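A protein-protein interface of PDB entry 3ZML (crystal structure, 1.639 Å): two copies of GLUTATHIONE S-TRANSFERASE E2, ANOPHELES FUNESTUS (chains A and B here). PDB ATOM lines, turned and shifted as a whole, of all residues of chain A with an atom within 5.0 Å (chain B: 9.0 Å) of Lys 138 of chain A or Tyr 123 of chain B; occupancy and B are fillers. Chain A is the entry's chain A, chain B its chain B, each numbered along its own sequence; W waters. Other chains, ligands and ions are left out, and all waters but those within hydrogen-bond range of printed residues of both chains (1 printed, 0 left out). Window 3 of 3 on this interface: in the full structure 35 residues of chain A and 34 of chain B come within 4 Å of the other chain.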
ATOM      1  N   ARG A 112     -31.599  -7.721   4.468  1.00  0.00           N
ATOM      2  CA  ARG A 112     -31.578  -8.448   3.175  1.00  0.00           C
ATOM      3  C   ARG A 112     -32.075  -7.560   2.040  1.00  0.00           C
ATOM      4  O   ARG A 112     -31.561  -7.693   0.930  1.00  0.00           O
ATOM      5  CB  ARG A 112     -32.349  -9.796   3.281  1.00  0.00           C
ATOM      6  CG  ARG A 112     -31.667 -10.685   4.316  1.00  0.00           C
ATOM      7  CD  ARG A 112     -32.519 -11.912   4.582  1.00  0.00           C
ATOM      8  NE  ARG A 112     -31.867 -12.715   5.631  1.00  0.00           N
ATOM      9  CZ  ARG A 112     -32.108 -14.016   5.847  1.00  0.00           C
ATOM     10  NH1 ARG A 112     -32.870 -14.708   5.047  1.00  0.00           N
ATOM     11  NH2 ARG A 112     -31.544 -14.690   6.884  1.00  0.00           N
ATOM     12  N   GLU A 134     -32.786 -15.178  -3.319  1.00  0.00           N
ATOM     13  CA  GLU A 134     -33.120 -16.322  -2.461  1.00  0.00           C
ATOM     14  C   GLU A 134     -33.141 -15.931  -0.978  1.00  0.00           C
ATOM     15  O   GLU A 134     -33.987 -16.330  -0.243  1.00  0.00           O
ATOM     16  CB  GLU A 134     -32.162 -17.483  -2.708  1.00  0.00           C
ATOM     17  CG  GLU A 134     -32.383 -18.661  -1.788  1.00  0.00           C
ATOM     18  CD  GLU A 134     -31.379 -19.789  -2.021  1.00  0.00           C
ATOM     19  OE1 GLU A 134     -30.203 -19.484  -2.285  1.00  0.00           O
ATOM     20  OE2 GLU A 134     -31.774 -20.967  -1.940  1.00  0.00           O
ATOM     21  N   TYR A 135     -32.193 -15.113  -0.571  1.00  0.00           N
ATOM     22  CA  TYR A 135     -32.115 -14.681   0.801  1.00  0.00           C
ATOM     23  C   TYR A 135     -33.406 -13.906   1.160  1.00  0.00           C
ATOM     24  O   TYR A 135     -33.939 -14.091   2.161  1.00  0.00           O
ATOM     25  CB  TYR A 135     -30.817 -13.856   0.985  1.00  0.00           C
ATOM     26  CG  TYR A 135     -30.039 -13.968   2.265  1.00  0.00           C
ATOM     27  CD1 TYR A 135     -29.974 -15.135   2.968  1.00  0.00           C
ATOM     28  CD2 TYR A 135     -29.360 -12.882   2.772  1.00  0.00           C
ATOM     29  CE1 TYR A 135     -29.284 -15.221   4.129  1.00  0.00           C
ATOM     30  CE2 TYR A 135     -28.625 -12.987   3.923  1.00  0.00           C
ATOM     31  CZ  TYR A 135     -28.612 -14.148   4.621  1.00  0.00           C
ATOM     32  OH  TYR A 135     -27.899 -14.241   5.817  1.00  0.00           O
ATOM     33  N   VAL A 136     -33.863 -13.054   0.240  1.00  0.00           N
ATOM     34  CA  VAL A 136     -35.107 -12.350   0.452  1.00  0.00           C
ATOM     35  C   VAL A 136     -36.328 -13.302   0.479  1.00  0.00           C
ATOM     36  O   VAL A 136     -37.136 -13.246   1.332  1.00  0.00           O
ATOM     37  CB  VAL A 136     -35.286 -11.168  -0.552  1.00  0.00           C
ATOM     38  CG1 VAL A 136     -36.703 -10.668  -0.547  1.00  0.00           C
ATOM     39  CG2 VAL A 136     -34.328 -10.046  -0.225  1.00  0.00           C
ATOM     40  N   GLN A 137     -36.386 -14.236  -0.441  1.00  0.00           N
ATOM     41  CA  GLN A 137     -37.517 -15.160  -0.404  1.00  0.00           C
ATOM     42  C   GLN A 137     -37.531 -15.946   0.907  1.00  0.00           C
ATOM     43  O   GLN A 137     -38.618 -16.240   1.434  1.00  0.00           O
ATOM     44  CB  GLN A 137     -37.446 -16.151  -1.555  1.00  0.00           C
ATOM     45  CG  GLN A 137     -37.719 -15.442  -2.915  1.00  0.00           C
ATOM     46  CD  GLN A 137     -37.225 -16.237  -4.125  1.00  0.00           C
ATOM     47  OE1 GLN A 137     -36.210 -16.969  -4.076  1.00  0.00           O
ATOM     48  NE2 GLN A 137     -37.917 -16.066  -5.241  1.00  0.00           N
ATOM     49  N   LYS A 138     -36.345 -16.272   1.437  1.00  0.00           N
ATOM     50  CA  LYS A 138     -36.293 -16.995   2.735  1.00  0.00           C
ATOM     51  C   LYS A 138     -36.846 -16.102   3.843  1.00  0.00           C
ATOM     52  O   LYS A 138     -37.640 -16.543   4.723  1.00  0.00           O
ATOM     53  CB  LYS A 138     -34.871 -17.488   3.064  1.00  0.00           C
ATOM     54  CG  LYS A 138     -34.457 -18.660   2.176  1.00  0.00           C
ATOM     55  CD  LYS A 138     -33.106 -19.149   2.657  1.00  0.00           C
ATOM     56  CE  LYS A 138     -32.866 -20.491   1.985  1.00  0.00           C
ATOM     57  NZ  LYS A 138     -31.767 -21.169   2.719  1.00  0.00           N
ATOM     58  N   SER A 139     -36.551 -14.814   3.747  1.00  0.00           N
ATOM     59  CA  SER A 139     -37.098 -13.856   4.751  1.00  0.00           C
ATOM     60  C   SER A 139     -38.640 -13.740   4.692  1.00  0.00           C
ATOM     61  O   SER A 139     -39.294 -13.578   5.706  1.00  0.00           O
ATOM     62  CB  SER A 139     -36.448 -12.455   4.620  1.00  0.00           C
ATOM     63  OG  SER A 139     -37.102 -11.600   3.599  1.00  0.00           O
ATOM     64  N   TYR A 140     -39.218 -13.899   3.496  1.00  0.00           N
ATOM     65  CA  TYR A 140     -40.658 -13.915   3.355  1.00  0.00           C
ATOM     66  C   TYR A 140     -41.258 -15.144   4.048  1.00  0.00           C
ATOM     67  O   TYR A 140     -42.211 -15.022   4.682  1.00  0.00           O
ATOM     68  CB  TYR A 140     -41.080 -13.942   1.894  1.00  0.00           C
ATOM     69  CG  TYR A 140     -40.770 -12.732   1.058  1.00  0.00           C
ATOM     70  CD1 TYR A 140     -40.518 -11.537   1.631  1.00  0.00           C
ATOM     71  CD2 TYR A 140     -40.782 -12.788  -0.329  1.00  0.00           C
ATOM     72  CE1 TYR A 140     -40.263 -10.433   0.869  1.00  0.00           C
ATOM     73  CE2 TYR A 140     -40.531 -11.678  -1.080  1.00  0.00           C
ATOM     74  CZ  TYR A 140     -40.308 -10.503  -0.484  1.00  0.00           C
ATOM     75  OH  TYR A 140     -40.097  -9.426  -1.294  1.00  0.00           O
ATOM     76  N   ARG A 141     -40.643 -16.300   3.888  1.00  0.00           N
ATOM     77  CA  ARG A 141     -41.124 -17.526   4.548  1.00  0.00           C
ATOM     78  C   ARG A 141     -41.062 -17.354   6.067  1.00  0.00           C
ATOM     79  O   ARG A 141     -42.020 -17.717   6.785  1.00  0.00           O
ATOM     80  CB  ARG A 141     -40.390 -18.781   4.060  1.00  0.00           C
ATOM     81  CG  ARG A 141     -40.756 -20.073   4.800  1.00  0.00           C
ATOM     82  CD  ARG A 141     -42.229 -20.482   4.650  1.00  0.00           C
ATOM     83  NE  ARG A 141     -42.611 -20.534   3.241  1.00  0.00           N
ATOM     84  CZ  ARG A 141     -43.840 -20.307   2.765  1.00  0.00           C
ATOM     85  NH1 ARG A 141     -44.847 -20.035   3.581  1.00  0.00           N
ATOM     86  NH2 ARG A 141     -44.068 -20.381   1.460  1.00  0.00           N
ATOM     87  N   LEU A 142     -39.963 -16.742   6.541  1.00  0.00           N
ATOM     88  CA  LEU A 142     -39.792 -16.549   8.002  1.00  0.00           C
ATOM     89  C   LEU A 142     -40.906 -15.671   8.562  1.00  0.00           C
ATOM     90  O   LEU A 142     -41.478 -15.965   9.626  1.00  0.00           O
ATOM     91  CB  LEU A 142     -38.414 -15.967   8.274  1.00  0.00           C
ATOM     92  CG  LEU A 142     -37.221 -16.899   8.020  1.00  0.00           C
ATOM     93  CD1 LEU A 142     -35.915 -16.118   7.979  1.00  0.00           C
ATOM     94  CD2 LEU A 142     -37.237 -17.973   9.123  1.00  0.00           C
ATOM     95  N   LEU B  38     -26.529 -26.840  15.245  1.00  0.00           N
ATOM     96  CA  LEU B  38     -27.044 -26.310  13.987  1.00  0.00           C
ATOM     97  C   LEU B  38     -26.506 -27.101  12.813  1.00  0.00           C
ATOM     98  O   LEU B  38     -27.220 -27.320  11.842  1.00  0.00           O
ATOM     99  CB  LEU B  38     -26.551 -24.849  13.825  1.00  0.00           C
ATOM    100  CG  LEU B  38     -27.102 -23.883  14.915  1.00  0.00           C
ATOM    101  CD1 LEU B  38     -26.524 -22.497  14.623  1.00  0.00           C
ATOM    102  CD2 LEU B  38     -28.641 -23.864  14.885  1.00  0.00           C
ATOM    103  N   LEU B  39     -25.251 -27.534  12.921  1.00  0.00           N
ATOM    104  CA  LEU B  39     -24.670 -28.282  11.764  1.00  0.00           C
ATOM    105  C   LEU B  39     -25.426 -29.607  11.533  1.00  0.00           C
ATOM    106  O   LEU B  39     -25.610 -30.025  10.391  1.00  0.00           O
ATOM    107  CB  LEU B  39     -23.202 -28.578  11.976  1.00  0.00           C
ATOM    108  CG  LEU B  39     -22.361 -27.298  11.957  1.00  0.00           C
ATOM    109  CD1 LEU B  39     -21.017 -27.725  12.529  1.00  0.00           C
ATOM    110  CD2 LEU B  39     -22.277 -26.656  10.548  1.00  0.00           C
ATOM    111  N   HIS B  43     -32.046 -27.460  14.899  1.00  0.00           N
ATOM    112  CA  HIS B  43     -32.986 -26.335  14.878  1.00  0.00           C
ATOM    113  C   HIS B  43     -34.066 -26.462  13.819  1.00  0.00           C
ATOM    114  O   HIS B  43     -34.874 -25.605  13.708  1.00  0.00           O
ATOM    115  CB  HIS B  43     -32.243 -25.019  14.636  1.00  0.00           C
ATOM    116  CG  HIS B  43     -31.407 -25.056  13.400  1.00  0.00           C
ATOM    117  ND1 HIS B  43     -31.464 -24.097  12.410  1.00  0.00           N
ATOM    118  CD2 HIS B  43     -30.523 -25.978  12.977  1.00  0.00           C
ATOM    119  CE1 HIS B  43     -30.638 -24.426  11.442  1.00  0.00           C
ATOM    120  NE2 HIS B  43     -30.063 -25.568  11.762  1.00  0.00           N
ATOM    121  N   LEU B  44     -33.999 -27.490  12.988  1.00  0.00           N
ATOM    122  CA  LEU B  44     -34.965 -27.571  11.848  1.00  0.00           C
ATOM    123  C   LEU B  44     -36.044 -28.654  12.086  1.00  0.00           C
ATOM    124  O   LEU B  44     -36.826 -28.953  11.186  1.00  0.00           O
ATOM    125  CB  LEU B  44     -34.239 -27.793  10.536  1.00  0.00           C
ATOM    126  CG  LEU B  44     -33.188 -26.699  10.300  1.00  0.00           C
ATOM    127  CD1 LEU B  44     -32.262 -27.093   9.143  1.00  0.00           C
ATOM    128  CD2 LEU B  44     -33.905 -25.384  10.038  1.00  0.00           C
ATOM    129  N   PRO B  53     -40.647 -20.185  15.342  1.00  0.00           N
ATOM    130  CA  PRO B  53     -40.929 -20.501  13.937  1.00  0.00           C
ATOM    131  C   PRO B  53     -39.845 -19.947  12.984  1.00  0.00           C
ATOM    132  O   PRO B  53     -39.792 -20.370  11.826  1.00  0.00           O
ATOM    133  CB  PRO B  53     -42.274 -19.785  13.694  1.00  0.00           C
ATOM    134  CG  PRO B  53     -42.249 -18.613  14.628  1.00  0.00           C
ATOM    135  CD  PRO B  53     -41.472 -19.053  15.846  1.00  0.00           C
ATOM    136  N   GLN B  54     -38.987 -19.035  13.451  1.00  0.00           N
ATOM    137  CA  GLN B  54     -37.839 -18.556  12.667  1.00  0.00           C
ATOM    138  C   GLN B  54     -36.622 -19.522  12.753  1.00  0.00           C
ATOM    139  O   GLN B  54     -35.602 -19.352  12.057  1.00  0.00           O
ATOM    140  CB  GLN B  54     -37.450 -17.152  13.087  1.00  0.00           C
ATOM    141  CG  GLN B  54     -38.509 -16.112  12.717  1.00  0.00           C
ATOM    142  CD  GLN B  54     -38.424 -14.861  13.576  1.00  0.00           C
ATOM    143  OE1 GLN B  54     -37.352 -14.525  14.122  1.00  0.00           O
ATOM    144  NE2 GLN B  54     -39.534 -14.131  13.673  1.00  0.00           N
ATOM    145  N   HIS B  55     -36.785 -20.561  13.579  1.00  0.00           N
ATOM    146  CA  HIS B  55     -35.757 -21.601  13.807  1.00  0.00           C
ATOM    147  C   HIS B  55     -34.356 -21.071  14.033  1.00  0.00           C
ATOM    148  O   HIS B  55     -33.393 -21.554  13.428  1.00  0.00           O
ATOM    149  CB  HIS B  55     -35.761 -22.691  12.704  1.00  0.00           C
ATOM    150  CG  HIS B  55     -35.703 -22.175  11.308  1.00  0.00           C
ATOM    151  ND1 HIS B  55     -34.559 -21.714  10.755  1.00  0.00           N
ATOM    152  CD2 HIS B  55     -36.666 -22.126  10.304  1.00  0.00           C
ATOM    153  CE1 HIS B  55     -34.778 -21.385   9.465  1.00  0.00           C
ATOM    154  NE2 HIS B  55     -36.068 -21.606   9.189  1.00  0.00           N
ATOM    155  N   ARG B 114     -23.091 -12.734   9.141  1.00  0.00           N
ATOM    156  CA  ARG B 114     -23.794 -13.920   8.761  1.00  0.00           C
ATOM    157  C   ARG B 114     -23.767 -14.075   7.212  1.00  0.00           C
ATOM    158  O   ARG B 114     -23.839 -15.185   6.673  1.00  0.00           O
ATOM    159  CB  ARG B 114     -25.220 -13.879   9.301  1.00  0.00           C
ATOM    160  CG  ARG B 114     -26.033 -15.093   8.862  1.00  0.00           C
ATOM    161  CD  ARG B 114     -27.392 -15.174   9.637  1.00  0.00           C
ATOM    162  NE  ARG B 114     -28.316 -16.095   8.902  1.00  0.00           N
ATOM    163  CZ  ARG B 114     -29.265 -16.871   9.424  1.00  0.00           C
ATOM    164  NH1 ARG B 114     -29.527 -16.859  10.756  1.00  0.00           N
ATOM    165  NH2 ARG B 114     -29.985 -17.682   8.599  1.00  0.00           N
ATOM    166  N   ILE B 116     -21.343 -13.597   5.419  1.00  0.00           N
ATOM    167  CA  ILE B 116     -20.138 -14.381   5.055  1.00  0.00           C
ATOM    168  C   ILE B 116     -20.213 -15.812   5.635  1.00  0.00           C
ATOM    169  O   ILE B 116     -19.880 -16.807   4.982  1.00  0.00           O
ATOM    170  CB  ILE B 116     -18.836 -13.659   5.494  1.00  0.00           C
ATOM    171  CG1 ILE B 116     -18.676 -12.374   4.687  1.00  0.00           C
ATOM    172  CG2 ILE B 116     -17.624 -14.596   5.360  1.00  0.00           C
ATOM    173  CD1 ILE B 116     -17.564 -11.472   5.236  1.00  0.00           C
ATOM    174  N   PHE B 117     -20.712 -15.915   6.849  1.00  0.00           N
ATOM    175  CA  PHE B 117     -20.482 -17.176   7.584  1.00  0.00           C
ATOM    176  C   PHE B 117     -21.486 -18.258   7.214  1.00  0.00           C
ATOM    177  O   PHE B 117     -21.151 -19.445   7.102  1.00  0.00           O
ATOM    178  CB  PHE B 117     -20.659 -16.951   9.114  1.00  0.00           C
ATOM    179  CG  PHE B 117     -19.477 -16.396   9.828  1.00  0.00           C
ATOM    180  CD1 PHE B 117     -18.422 -15.757   9.143  1.00  0.00           C
ATOM    181  CD2 PHE B 117     -19.436 -16.472  11.227  1.00  0.00           C
ATOM    182  CE1 PHE B 117     -17.337 -15.178   9.840  1.00  0.00           C
ATOM    183  CE2 PHE B 117     -18.388 -15.907  11.925  1.00  0.00           C
ATOM    184  CZ  PHE B 117     -17.301 -15.305  11.263  1.00  0.00           C
ATOM    185  N   GLU B 118     -22.772 -17.912   7.020  1.00  0.00           N
ATOM    186  CA  GLU B 118     -23.823 -18.903   6.848  1.00  0.00           C
ATOM    187  C   GLU B 118     -23.548 -19.788   5.639  1.00  0.00           C
ATOM    188  O   GLU B 118     -23.671 -21.001   5.720  1.00  0.00           O
ATOM    189  CB  GLU B 118     -25.206 -18.244   6.650  1.00  0.00           C
ATOM    190  CG  GLU B 118     -26.348 -19.236   6.447  1.00  0.00           C
ATOM    191  CD  GLU B 118     -27.699 -18.588   6.327  1.00  0.00           C
ATOM    192  OE1 GLU B 118     -27.798 -17.357   6.136  1.00  0.00           O
ATOM    193  OE2 GLU B 118     -28.674 -19.354   6.523  1.00  0.00           O
ATOM    194  N   ARG B 119     -23.198 -19.141   4.525  1.00  0.00           N
ATOM    195  CA  ARG B 119     -23.010 -19.911   3.275  1.00  0.00           C
ATOM    196  C   ARG B 119     -21.844 -20.890   3.361  1.00  0.00           C
ATOM    197  O   ARG B 119     -21.875 -21.929   2.724  1.00  0.00           O
ATOM    198  CB  ARG B 119     -22.916 -18.947   2.081  1.00  0.00           C
ATOM    199  CG  ARG B 119     -21.677 -18.020   2.124  1.00  0.00           C
ATOM    200  CD  ARG B 119     -21.859 -16.765   1.269  1.00  0.00           C
ATOM    201  NE  ARG B 119     -21.957 -17.118  -0.157  1.00  0.00           N
ATOM    202  CZ  ARG B 119     -20.843 -17.375  -0.867  1.00  0.00           C
ATOM    203  NH1 ARG B 119     -19.640 -17.368  -0.295  1.00  0.00           N
ATOM    204  NH2 ARG B 119     -20.908 -17.690  -2.162  1.00  0.00           N
ATOM    205  N   ILE B 120     -20.841 -20.572   4.173  1.00  0.00           N
ATOM    206  CA  ILE B 120     -19.689 -21.468   4.377  1.00  0.00           C
ATOM    207  C   ILE B 120     -20.091 -22.570   5.326  1.00  0.00           C
ATOM    208  O   ILE B 120     -19.907 -23.751   5.029  1.00  0.00           O
ATOM    209  CB  ILE B 120     -18.483 -20.719   4.909  1.00  0.00           C
ATOM    210  CG1 ILE B 120     -17.882 -19.779   3.838  1.00  0.00           C
ATOM    211  CG2 ILE B 120     -17.371 -21.664   5.476  1.00  0.00           C
ATOM    212  CD1 ILE B 120     -16.913 -18.742   4.394  1.00  0.00           C
ATOM    213  N   LEU B 121     -20.697 -22.195   6.464  1.00  0.00           N
ATOM    214  CA  LEU B 121     -21.039 -23.194   7.505  1.00  0.00           C
ATOM    215  C   LEU B 121     -22.076 -24.235   7.063  1.00  0.00           C
ATOM    216  O   LEU B 121     -21.935 -25.419   7.358  1.00  0.00           O
ATOM    217  CB  LEU B 121     -21.552 -22.469   8.753  1.00  0.00           C
ATOM    218  CG  LEU B 121     -20.469 -21.651   9.503  1.00  0.00           C
ATOM    219  CD1 LEU B 121     -21.142 -20.831  10.605  1.00  0.00           C
ATOM    220  CD2 LEU B 121     -19.351 -22.535  10.046  1.00  0.00           C
ATOM    221  N   PHE B 122     -23.081 -23.815   6.294  1.00  0.00           N
ATOM    222  CA  PHE B 122     -24.258 -24.639   6.033  1.00  0.00           C
ATOM    223  C   PHE B 122     -24.523 -25.001   4.555  1.00  0.00           C
ATOM    224  O   PHE B 122     -25.280 -25.951   4.274  1.00  0.00           O
ATOM    225  CB  PHE B 122     -25.475 -23.963   6.614  1.00  0.00           C
ATOM    226  CG  PHE B 122     -25.333 -23.688   8.070  1.00  0.00           C
ATOM    227  CD1 PHE B 122     -25.380 -24.739   8.979  1.00  0.00           C
ATOM    228  CD2 PHE B 122     -25.151 -22.378   8.566  1.00  0.00           C
ATOM    229  CE1 PHE B 122     -25.253 -24.512  10.352  1.00  0.00           C
ATOM    230  CE2 PHE B 122     -25.014 -22.152   9.938  1.00  0.00           C
ATOM    231  CZ  PHE B 122     -25.052 -23.206  10.826  1.00  0.00           C
ATOM    232  N   TYR B 123     -23.957 -24.259   3.610  1.00  0.00           N
ATOM    233  CA  TYR B 123     -24.318 -24.390   2.207  1.00  0.00           C
ATOM    234  C   TYR B 123     -23.095 -24.672   1.311  1.00  0.00           C
ATOM    235  O   TYR B 123     -23.181 -24.540   0.071  1.00  0.00           O
ATOM    236  CB  TYR B 123     -25.102 -23.189   1.718  1.00  0.00           C
ATOM    237  CG  TYR B 123     -26.420 -23.058   2.471  1.00  0.00           C
ATOM    238  CD1 TYR B 123     -27.394 -24.065   2.339  1.00  0.00           C
ATOM    239  CD2 TYR B 123     -26.639 -22.016   3.390  1.00  0.00           C
ATOM    240  CE1 TYR B 123     -28.566 -24.024   3.070  1.00  0.00           C
ATOM    241  CE2 TYR B 123     -27.830 -21.958   4.135  1.00  0.00           C
ATOM    242  CZ  TYR B 123     -28.781 -22.947   3.943  1.00  0.00           C
ATOM    243  OH  TYR B 123     -29.954 -22.918   4.670  1.00  0.00           O
ATOM    244  N   GLY B 124     -21.986 -25.050   1.955  1.00  0.00           N
ATOM    245  CA  GLY B 124     -20.849 -25.605   1.250  1.00  0.00           C
ATOM    246  C   GLY B 124     -19.965 -24.661   0.474  1.00  0.00           C
ATOM    247  O   GLY B 124     -19.142 -25.106  -0.374  1.00  0.00           O
ATOM    248  N   LYS B 125     -20.129 -23.361   0.668  1.00  0.00           N
ATOM    249  CA  LYS B 125     -19.335 -22.423  -0.115  1.00  0.00           C
ATOM    250  C   LYS B 125     -17.882 -22.363   0.363  1.00  0.00           C
ATOM    251  O   LYS B 125     -17.543 -22.531   1.576  1.00  0.00           O
ATOM    252  CB  LYS B 125     -19.948 -20.998  -0.202  1.00  0.00           C
ATOM    253  CG  LYS B 125     -21.451 -20.940  -0.591  1.00  0.00           C
ATOM    254  CD  LYS B 125     -21.726 -21.663  -1.917  1.00  0.00           C
ATOM    255  CE  LYS B 125     -23.222 -21.791  -2.154  1.00  0.00           C
ATOM    256  NZ  LYS B 125     -23.573 -22.103  -3.579  1.00  0.00           N
ATOM    257  N   SER B 126     -16.983 -22.169  -0.610  1.00  0.00           N
ATOM    258  CA  SER B 126     -15.564 -22.103  -0.304  1.00  0.00           C
ATOM    259  C   SER B 126     -14.906 -20.765  -0.528  1.00  0.00           C
ATOM    260  O   SER B 126     -13.724 -20.645  -0.386  1.00  0.00           O
ATOM    261  CB  SER B 126     -14.808 -23.157  -1.126  1.00  0.00           C
ATOM    262  OG  SER B 126     -14.986 -22.793  -2.455  1.00  0.00           O
ATOM    263  N   ASP B 127     -15.663 -19.733  -0.855  1.00  0.00           N
ATOM    264  CA  ASP B 127     -15.050 -18.438  -1.068  1.00  0.00           C
ATOM    265  C   ASP B 127     -15.587 -17.412  -0.068  1.00  0.00           C
ATOM    266  O   ASP B 127     -16.647 -17.644   0.603  1.00  0.00           O
ATOM    267  CB  ASP B 127     -15.302 -17.960  -2.512  1.00  0.00           C
ATOM    268  CG  ASP B 127     -16.799 -17.819  -2.864  1.00  0.00           C
ATOM    269  OD1 ASP B 127     -17.711 -18.490  -2.321  1.00  0.00           O
ATOM    270  OD2 ASP B 127     -17.095 -17.034  -3.805  1.00  0.00           O
ATOM    271  N   LYS B 216     -13.769 -24.728   7.800  1.00  0.00           N
ATOM    272  CA  LYS B 216     -14.882 -25.258   7.067  1.00  0.00           C
ATOM    273  C   LYS B 216     -14.784 -24.739   5.606  1.00  0.00           C
ATOM    274  O   LYS B 216     -15.139 -25.502   4.683  1.00  0.00           O
ATOM    275  CB  LYS B 216     -16.144 -24.801   7.779  1.00  0.00           C
ATOM    276  CG  LYS B 216     -17.413 -25.282   7.169  1.00  0.00           C
ATOM    277  CD  LYS B 216     -17.566 -26.794   7.436  1.00  0.00           C
ATOM    278  CE  LYS B 216     -18.664 -27.291   6.525  1.00  0.00           C
ATOM    279  NZ  LYS B 216     -19.211 -28.619   6.936  1.00  0.00           N
ATOM    280  N   ASN B 220     -14.654 -27.264   2.505  1.00  0.00           N
ATOM    281  CA  ASN B 220     -15.693 -27.249   1.463  1.00  0.00           C
ATOM    282  C   ASN B 220     -15.010 -27.274   0.091  1.00  0.00           C
ATOM    283  O   ASN B 220     -15.577 -27.807  -0.897  1.00  0.00           O
ATOM    284  CB  ASN B 220     -16.513 -25.945   1.585  1.00  0.00           C
ATOM    285  CG  ASN B 220     -17.485 -25.979   2.743  1.00  0.00           C
ATOM    286  OD1 ASN B 220     -17.721 -27.030   3.353  1.00  0.00           O
ATOM    287  ND2 ASN B 220     -18.036 -24.792   3.083  1.00  0.00           N
HETATM  288  O   HOH W   1     -30.343 -13.690   9.063  1.00  0.00           O
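No position is printed for both chains.
Of the 6 pairs that touch across the chains among the printed residues, none has its exchanged pair printed and touching as well.
Water W1 lies within hydrogen-bond range of the guanidinium group of Arg 112 of chain A and the guanidinium group of Arg 114 of chain B.
OE2 of Glu 118 of chain B lies within salt-bridge range of NH2 of Arg 114 of chain B.
The guanidinium group (NH1) of Arg 112 of chain A is in hydrogen-bond range of the backbone carbonyl oxygen (O) of Tyr 135 of chain A (3.1 Å).
A ring nitrogen (ND1) of His 43 of chain B is in hydrogen-bond range of the backbone carbonyl oxygen (O) of His 55 of chain B, at 3.4 Å.
Of the 10 printed residues of chain A, 4 touch a printed residue of chain B.
Hydrophobic or aromatic side chains of chain A that line the printed part of chain B: Tyr 135 and Leu 142.
Printed residues of chain B that touch a printed residue of chain A: Gln 54, His 55, Arg 114, Glu 118 and Tyr 123.
Among the printed residues, 6 pairs touch across the chains.
Among the printed residues, no Asp or Glu carboxylate lies within 4 Å of a Lys or Arg side-chain nitrogen of the other chain.
The side-chain carboxylate of Glu 118 of chain B is in hydrogen-bond range of the side-chain hydroxyl of Tyr 135 of chain A (3.1 Å).
NZ of Lys 138 of chain A sits at hydrogen-bond distance from OH of Tyr 123 of chain B, 3.2 Å away.
Of chain A, only Lys 138 (3.2 Å) comes within 4 Å of Tyr 123 of chain B.
No residue of chain B comes within 4 Å of Ser 139 of chain A.
Printed residues of chain B within 4 Å of Arg 112 of chain A: Arg 114.
Printed residues of chain A within 4 Å of His 55 of chain B: Leu 142.
Of the printed residues of chain A, Glu 118 of chain B touches Tyr 135 (3.1 Å).
Of the printed residues of chain A, Arg 114 of chain B touches Arg 112 (3.8 Å) and Tyr 135 (3.6 Å).
Of the printed residues of chain A, Gln 54 of chain B touches Leu 142.
Asn 220 of chain B touches none of the printed residues of chain A.
The nearest residue of chain B that does not touch Lys 138 of chain A is Glu 118 of chain B (5.2 Å).
The nearest printed residue of chain B that does not touch Tyr 135 of chain A is Ile 116 of chain B (6.6 Å).
Arg 112 of chain A touches Arg 114 of chain B (NH2 to NH2, 3.8 Å).
Tyr 135 of chain A touches Arg 114 of chain B (OH to NE, 3.6 Å).
Leu 142 of chain A touches Gln 54 of chain B (CD2 to O, 3.6 Å).
CD2 of Leu 142 of chain A touches NE2 of His 55 of chain B (3.8 Å).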
